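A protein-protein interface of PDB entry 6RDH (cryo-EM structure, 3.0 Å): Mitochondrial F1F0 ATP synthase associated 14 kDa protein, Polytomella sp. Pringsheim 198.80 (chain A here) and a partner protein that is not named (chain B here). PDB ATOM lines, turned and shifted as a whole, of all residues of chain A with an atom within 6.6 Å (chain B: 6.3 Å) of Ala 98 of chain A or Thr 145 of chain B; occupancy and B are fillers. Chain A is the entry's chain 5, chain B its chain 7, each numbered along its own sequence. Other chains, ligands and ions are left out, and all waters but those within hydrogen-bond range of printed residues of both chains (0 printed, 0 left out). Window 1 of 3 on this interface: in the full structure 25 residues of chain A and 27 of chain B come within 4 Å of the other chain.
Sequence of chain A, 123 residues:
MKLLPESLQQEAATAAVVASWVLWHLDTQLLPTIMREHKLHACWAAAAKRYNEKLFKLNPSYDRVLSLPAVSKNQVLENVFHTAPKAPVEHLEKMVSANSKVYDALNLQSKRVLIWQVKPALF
Among the printed residues, pairs that only touch across the chains: Met 95 of chain A with Tyr 141 of chain B (3.7 Å), Ala 98 of chain A with Tyr 141 of chain B (3.6 Å), Ala 98 of chain A with Thr 145 of chain B (3.7 Å), Lys 101 of chain A with Thr 145 of chain B (3.3 Å), Val 102 of chain A with Thr 145 of chain B (3.6 Å) and Ala 105 of chain A with Phe 147 of chain B (3.5 Å).
Of the 10 printed residues of chain B, 5 touch a printed residue of chain A.
Hydrophobic or aromatic side chains of chain B that line the printed part of chain A: Tyr 141 and Phe 147.
Of the 12 printed residues of chain A, 7 touch a printed residue of chain B.
Hydrophobic or aromatic side chains of chain A within 4 Å of the printed part of chain B: Met 95, Ala 98, Val 102 and Ala 105.
O of Lys 94 of chain A sits at hydrogen-bond distance from OG of Ser 97 of chain A, at 2.6 Å.
The backbone carbonyl oxygen of Met 95 of chain A sits close to the side-chain amide nitrogen of Asn 99 of chain A, at 3.3 Å.
The backbone carbonyl oxygen (O) of Tyr 141 of chain B sits at hydrogen-bond distance from the side-chain hydroxyl (OG1) of Thr 145 of chain B (2.9 Å).
Printed residues of chain B within 4 Å of Lys 94 of chain A: Glu 142 (3.3 Å).
Of the printed residues of chain B, Met 95 of chain A touches Tyr 141 (3.7 Å).
Printed residues of chain B within 4 Å of Ala 98 of chain A: Tyr 141 (3.6 Å) and Thr 145 (3.7 Å).
Tyr 103 of chain A touches none of the printed residues of chain B.
Thr 145 of chain B touches just these residues of chain A: Ala 98, Lys 101 and Val 102.
The nearest residue of chain B that does not touch Ala 98 of chain A is Glu 142 of chain B (4.4 Å).
The side-chain amino group (NZ) of Lys 94 of chain A is in salt-bridge range of the side-chain carboxylate (OE2) of Glu 142 of chain B (3.3 Å).
O of Glu 142 of chain B is in hydrogen-bond range of NZ of Lys 101 of chain A (3.0 Å).
The side-chain carboxylate (OE1) of Glu 146 of chain B is in salt-bridge range of the side-chain amino group (NZ) of Lys 101 of chain A.
OD1 of Asn 99 of chain A lies close to OH of Tyr 141 of chain B (2.4 Å).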
ATOM      1  N   GLU A  93       2.376   1.540 -32.984  1.00  0.00           N
ATOM      2  CA  GLU A  93       1.788   1.389 -31.655  1.00  0.00           C
ATOM      3  C   GLU A  93       2.823   0.960 -30.622  1.00  0.00           C
ATOM      4  O   GLU A  93       2.907   1.549 -29.539  1.00  0.00           O
ATOM      5  CB  GLU A  93       0.630   0.396 -31.701  1.00  0.00           C
ATOM      6  CG  GLU A  93      -0.584   0.912 -32.438  1.00  0.00           C
ATOM      7  CD  GLU A  93      -1.689   1.358 -31.509  1.00  0.00           C
ATOM      8  OE1 GLU A  93      -1.599   1.081 -30.297  1.00  0.00           O
ATOM      9  OE2 GLU A  93      -2.649   1.994 -31.991  1.00  0.00           O
ATOM     10  N   LYS A  94       3.666  -0.015 -30.968  1.00  0.00           N
ATOM     11  CA  LYS A  94       4.658  -0.515 -30.025  1.00  0.00           C
ATOM     12  C   LYS A  94       5.756   0.508 -29.768  1.00  0.00           C
ATOM     13  O   LYS A  94       6.106   0.780 -28.610  1.00  0.00           O
ATOM     14  CB  LYS A  94       5.256  -1.815 -30.545  1.00  0.00           C
ATOM     15  CG  LYS A  94       4.299  -2.974 -30.487  1.00  0.00           C
ATOM     16  CD  LYS A  94       5.027  -4.288 -30.520  1.00  0.00           C
ATOM     17  CE  LYS A  94       4.226  -5.337 -29.802  1.00  0.00           C
ATOM     18  NZ  LYS A  94       3.872  -4.879 -28.440  1.00  0.00           N
ATOM     19  N   MET A  95       6.296   1.111 -30.828  1.00  0.00           N
ATOM     20  CA  MET A  95       7.383   2.051 -30.627  1.00  0.00           C
ATOM     21  C   MET A  95       6.895   3.370 -30.048  1.00  0.00           C
ATOM     22  O   MET A  95       7.659   4.044 -29.364  1.00  0.00           O
ATOM     23  CB  MET A  95       8.128   2.280 -31.930  1.00  0.00           C
ATOM     24  CG  MET A  95       8.765   1.044 -32.499  1.00  0.00           C
ATOM     25  SD  MET A  95      10.162   0.437 -31.564  1.00  0.00           S
ATOM     26  CE  MET A  95      11.440   1.501 -32.197  1.00  0.00           C
ATOM     27  N   VAL A  96       5.632   3.742 -30.254  1.00  0.00           N
ATOM     28  CA  VAL A  96       5.116   4.936 -29.601  1.00  0.00           C
ATOM     29  C   VAL A  96       4.838   4.665 -28.130  1.00  0.00           C
ATOM     30  O   VAL A  96       5.100   5.523 -27.279  1.00  0.00           O
ATOM     31  CB  VAL A  96       3.886   5.446 -30.373  1.00  0.00           C
ATOM     32  CG1 VAL A  96       2.949   6.247 -29.504  1.00  0.00           C
ATOM     33  CG2 VAL A  96       4.343   6.311 -31.520  1.00  0.00           C
ATOM     34  N   SER A  97       4.391   3.453 -27.787  1.00  0.00           N
ATOM     35  CA  SER A  97       4.229   3.113 -26.378  1.00  0.00           C
ATOM     36  C   SER A  97       5.558   3.050 -25.643  1.00  0.00           C
ATOM     37  O   SER A  97       5.600   3.296 -24.437  1.00  0.00           O
ATOM     38  CB  SER A  97       3.518   1.778 -26.224  1.00  0.00           C
ATOM     39  OG  SER A  97       4.368   0.723 -26.615  1.00  0.00           O
ATOM     40  N   ALA A  98       6.644   2.714 -26.334  1.00  0.00           N
ATOM     41  CA  ALA A  98       7.951   2.727 -25.681  1.00  0.00           C
ATOM     42  C   ALA A  98       8.611   4.098 -25.685  1.00  0.00           C
ATOM     43  O   ALA A  98       9.241   4.497 -24.691  1.00  0.00           O
ATOM     44  CB  ALA A  98       8.876   1.721 -26.348  1.00  0.00           C
ATOM     45  N   ASN A  99       8.463   4.863 -26.757  1.00  0.00           N
ATOM     46  CA  ASN A  99       8.989   6.211 -26.739  1.00  0.00           C
ATOM     47  C   ASN A  99       8.164   7.141 -25.874  1.00  0.00           C
ATOM     48  O   ASN A  99       8.627   8.238 -25.582  1.00  0.00           O
ATOM     49  CB  ASN A  99       9.081   6.765 -28.150  1.00  0.00           C
ATOM     50  CG  ASN A  99      10.066   6.019 -29.001  1.00  0.00           C
ATOM     51  OD1 ASN A  99      10.914   5.297 -28.498  1.00  0.00           O
ATOM     52  ND2 ASN A  99       9.960   6.189 -30.305  1.00  0.00           N
ATOM     53  N   SER A 100       6.977   6.729 -25.433  1.00  0.00           N
ATOM     54  CA  SER A 100       6.302   7.467 -24.375  1.00  0.00           C
ATOM     55  C   SER A 100       7.082   7.395 -23.074  1.00  0.00           C
ATOM     56  O   SER A 100       7.139   8.368 -22.323  1.00  0.00           O
ATOM     57  CB  SER A 100       4.895   6.927 -24.172  1.00  0.00           C
ATOM     58  OG  SER A 100       4.281   7.587 -23.090  1.00  0.00           O
ATOM     59  N   LYS A 101       7.711   6.255 -22.800  1.00  0.00           N
ATOM     60  CA  LYS A 101       8.556   6.145 -21.620  1.00  0.00           C
ATOM     61  C   LYS A 101       9.875   6.874 -21.814  1.00  0.00           C
ATOM     62  O   LYS A 101      10.426   7.432 -20.857  1.00  0.00           O
ATOM     63  CB  LYS A 101       8.796   4.679 -21.297  1.00  0.00           C
ATOM     64  CG  LYS A 101       7.578   3.976 -20.761  1.00  0.00           C
ATOM     65  CD  LYS A 101       7.387   2.641 -21.409  1.00  0.00           C
ATOM     66  CE  LYS A 101       8.591   1.766 -21.222  1.00  0.00           C
ATOM     67  NZ  LYS A 101       8.342   0.432 -21.794  1.00  0.00           N
ATOM     68  N   VAL A 102      10.395   6.869 -23.042  1.00  0.00           N
ATOM     69  CA  VAL A 102      11.565   7.697 -23.352  1.00  0.00           C
ATOM     70  C   VAL A 102      11.249   9.176 -23.166  1.00  0.00           C
ATOM     71  O   VAL A 102      12.088   9.949 -22.696  1.00  0.00           O
ATOM     72  CB  VAL A 102      12.067   7.414 -24.777  1.00  0.00           C
ATOM     73  CG1 VAL A 102      13.341   8.162 -25.066  1.00  0.00           C
ATOM     74  CG2 VAL A 102      12.301   5.972 -24.947  1.00  0.00           C
ATOM     75  N   TYR A 103      10.037   9.593 -23.524  1.00  0.00           N
ATOM     76  CA  TYR A 103       9.623  10.968 -23.293  1.00  0.00           C
ATOM     77  C   TYR A 103       9.493  11.253 -21.810  1.00  0.00           C
ATOM     78  O   TYR A 103      10.014  12.259 -21.321  1.00  0.00           O
ATOM     79  CB  TYR A 103       8.294  11.257 -23.993  1.00  0.00           C
ATOM     80  CG  TYR A 103       7.726  12.611 -23.638  1.00  0.00           C
ATOM     81  CD1 TYR A 103       8.182  13.743 -24.266  1.00  0.00           C
ATOM     82  CD2 TYR A 103       6.736  12.759 -22.673  1.00  0.00           C
ATOM     83  CE1 TYR A 103       7.687  14.961 -23.958  1.00  0.00           C
ATOM     84  CE2 TYR A 103       6.264  13.987 -22.337  1.00  0.00           C
ATOM     85  CZ  TYR A 103       6.738  15.081 -22.985  1.00  0.00           C
ATOM     86  OH  TYR A 103       6.252  16.312 -22.658  1.00  0.00           O
ATOM     87  N   ALA A 105      10.725   9.910 -19.170  1.00  0.00           N
ATOM     88  CA  ALA A 105      11.885   9.930 -18.303  1.00  0.00           C
ATOM     89  C   ALA A 105      12.858  11.050 -18.611  1.00  0.00           C
ATOM     90  O   ALA A 105      13.547  11.510 -17.702  1.00  0.00           O
ATOM     91  CB  ALA A 105      12.618   8.600 -18.373  1.00  0.00           C
ATOM     92  N   TYR B 101      20.881   1.287 -25.125  1.00  0.00           N
ATOM     93  CA  TYR B 101      19.979   1.953 -26.050  1.00  0.00           C
ATOM     94  C   TYR B 101      20.691   2.378 -27.320  1.00  0.00           C
ATOM     95  O   TYR B 101      20.080   2.389 -28.389  1.00  0.00           O
ATOM     96  CB  TYR B 101      19.369   3.160 -25.341  1.00  0.00           C
ATOM     97  CG  TYR B 101      18.438   4.053 -26.123  1.00  0.00           C
ATOM     98  CD1 TYR B 101      17.071   3.907 -26.021  1.00  0.00           C
ATOM     99  CD2 TYR B 101      18.923   5.095 -26.895  1.00  0.00           C
ATOM    100  CE1 TYR B 101      16.228   4.735 -26.700  1.00  0.00           C
ATOM    101  CE2 TYR B 101      18.090   5.908 -27.581  1.00  0.00           C
ATOM    102  CZ  TYR B 101      16.753   5.731 -27.477  1.00  0.00           C
ATOM    103  OH  TYR B 101      15.934   6.571 -28.164  1.00  0.00           O
ATOM    104  N   LEU B 140      13.129  -6.164 -26.492  1.00  0.00           N
ATOM    105  CA  LEU B 140      14.350  -5.518 -26.014  1.00  0.00           C
ATOM    106  C   LEU B 140      14.180  -4.012 -25.901  1.00  0.00           C
ATOM    107  O   LEU B 140      14.656  -3.398 -24.942  1.00  0.00           O
ATOM    108  CB  LEU B 140      15.518  -5.837 -26.941  1.00  0.00           C
ATOM    109  CG  LEU B 140      15.891  -7.303 -27.105  1.00  0.00           C
ATOM    110  CD1 LEU B 140      17.070  -7.442 -28.028  1.00  0.00           C
ATOM    111  CD2 LEU B 140      16.167  -7.943 -25.775  1.00  0.00           C
ATOM    112  N   TYR B 141      13.482  -3.403 -26.851  1.00  0.00           N
ATOM    113  CA  TYR B 141      13.278  -1.965 -26.805  1.00  0.00           C
ATOM    114  C   TYR B 141      12.246  -1.571 -25.765  1.00  0.00           C
ATOM    115  O   TYR B 141      12.331  -0.483 -25.198  1.00  0.00           O
ATOM    116  CB  TYR B 141      12.858  -1.454 -28.168  1.00  0.00           C
ATOM    117  CG  TYR B 141      12.906   0.036 -28.273  1.00  0.00           C
ATOM    118  CD1 TYR B 141      14.112   0.701 -28.369  1.00  0.00           C
ATOM    119  CD2 TYR B 141      11.749   0.779 -28.280  1.00  0.00           C
ATOM    120  CE1 TYR B 141      14.156   2.056 -28.467  1.00  0.00           C
ATOM    121  CE2 TYR B 141      11.789   2.134 -28.377  1.00  0.00           C
ATOM    122  CZ  TYR B 141      12.988   2.764 -28.469  1.00  0.00           C
ATOM    123  OH  TYR B 141      13.006   4.127 -28.565  1.00  0.00           O
ATOM    124  N   GLU B 142      11.257  -2.420 -25.503  1.00  0.00           N
ATOM    125  CA  GLU B 142      10.307  -2.093 -24.454  1.00  0.00           C
ATOM    126  C   GLU B 142      10.935  -2.222 -23.079  1.00  0.00           C
ATOM    127  O   GLU B 142      10.520  -1.530 -22.150  1.00  0.00           O
ATOM    128  CB  GLU B 142       9.073  -2.984 -24.562  1.00  0.00           C
ATOM    129  CG  GLU B 142       8.018  -2.489 -25.541  1.00  0.00           C
ATOM    130  CD  GLU B 142       6.971  -3.542 -25.860  1.00  0.00           C
ATOM    131  OE1 GLU B 142       7.162  -4.717 -25.485  1.00  0.00           O
ATOM    132  OE2 GLU B 142       5.954  -3.194 -26.491  1.00  0.00           O
ATOM    133  N   THR B 143      11.932  -3.093 -22.921  1.00  0.00           N
ATOM    134  CA  THR B 143      12.552  -3.216 -21.607  1.00  0.00           C
ATOM    135  C   THR B 143      13.773  -2.331 -21.407  1.00  0.00           C
ATOM    136  O   THR B 143      14.137  -2.084 -20.259  1.00  0.00           O
ATOM    137  CB  THR B 143      12.940  -4.664 -21.302  1.00  0.00           C
ATOM    138  OG1 THR B 143      13.428  -4.728 -19.967  1.00  0.00           O
ATOM    139  CG2 THR B 143      14.028  -5.154 -22.201  1.00  0.00           C
ATOM    140  N   VAL B 144      14.416  -1.831 -22.462  1.00  0.00           N
ATOM    141  CA  VAL B 144      15.548  -0.940 -22.217  1.00  0.00           C
ATOM    142  C   VAL B 144      15.072   0.476 -21.935  1.00  0.00           C
ATOM    143  O   VAL B 144      15.819   1.276 -21.366  1.00  0.00           O
ATOM    144  CB  VAL B 144      16.552  -0.961 -23.383  1.00  0.00           C
ATOM    145  CG1 VAL B 144      16.101  -0.094 -24.517  1.00  0.00           C
ATOM    146  CG2 VAL B 144      17.932  -0.572 -22.929  1.00  0.00           C
ATOM    147  N   THR B 145      13.828   0.799 -22.275  1.00  0.00           N
ATOM    148  CA  THR B 145      13.265   2.114 -22.031  1.00  0.00           C
ATOM    149  C   THR B 145      12.353   2.133 -20.820  1.00  0.00           C
ATOM    150  O   THR B 145      11.635   3.108 -20.613  1.00  0.00           O
ATOM    151  CB  THR B 145      12.518   2.596 -23.261  1.00  0.00           C
ATOM    152  OG1 THR B 145      11.422   1.724 -23.510  1.00  0.00           O
ATOM    153  CG2 THR B 145      13.420   2.537 -24.431  1.00  0.00           C
ATOM    154  N   GLU B 146      12.363   1.079 -20.013  1.00  0.00           N
ATOM    155  CA  GLU B 146      11.707   1.100 -18.713  1.00  0.00           C
ATOM    156  C   GLU B 146      12.675   1.748 -17.728  1.00  0.00           C
ATOM    157  O   GLU B 146      13.397   1.088 -16.980  1.00  0.00           O
ATOM    158  CB  GLU B 146      11.313  -0.307 -18.293  1.00  0.00           C
ATOM    159  CG  GLU B 146      10.470  -0.388 -17.044  1.00  0.00           C
ATOM    160  CD  GLU B 146       9.100   0.194 -17.234  1.00  0.00           C
ATOM    161  OE1 GLU B 146       8.535   0.013 -18.327  1.00  0.00           O
ATOM    162  OE2 GLU B 146       8.583   0.841 -16.299  1.00  0.00           O
ATOM    163  N   PHE B 147      12.710   3.081 -17.754  1.00  0.00           N
ATOM    164  CA  PHE B 147      13.593   3.831 -16.878  1.00  0.00           C
ATOM    165  C   PHE B 147      13.016   4.032 -15.488  1.00  0.00           C
ATOM    166  O   PHE B 147      13.726   4.527 -14.613  1.00  0.00           O
ATOM    167  CB  PHE B 147      13.923   5.195 -17.477  1.00  0.00           C
ATOM    168  CG  PHE B 147      14.546   5.134 -18.830  1.00  0.00           C
ATOM    169  CD1 PHE B 147      15.762   4.535 -19.017  1.00  0.00           C
ATOM    170  CD2 PHE B 147      13.913   5.689 -19.915  1.00  0.00           C
ATOM    171  CE1 PHE B 147      16.327   4.484 -20.267  1.00  0.00           C
ATOM    172  CE2 PHE B 147      14.473   5.648 -21.154  1.00  0.00           C
ATOM    173  CZ  PHE B 147      15.681   5.047 -21.330  1.00  0.00           C
ATOM    174  N   ASP B 148      11.760   3.675 -15.257  1.00  0.00           N
ATOM    175  CA  ASP B 148      11.213   3.658 -13.907  1.00  0.00           C
ATOM    176  C   ASP B 148      11.559   2.388 -13.148  1.00  0.00           C
ATOM    177  O   ASP B 148      11.013   2.158 -12.069  1.00  0.00           O
ATOM    178  CB  ASP B 148       9.696   3.820 -13.931  1.00  0.00           C
ATOM    179  CG  ASP B 148       9.261   5.219 -14.284  1.00  0.00           C
ATOM    180  OD1 ASP B 148      10.030   6.166 -14.041  1.00  0.00           O
ATOM    181  OD2 ASP B 148       8.129   5.378 -14.779  1.00  0.00           O
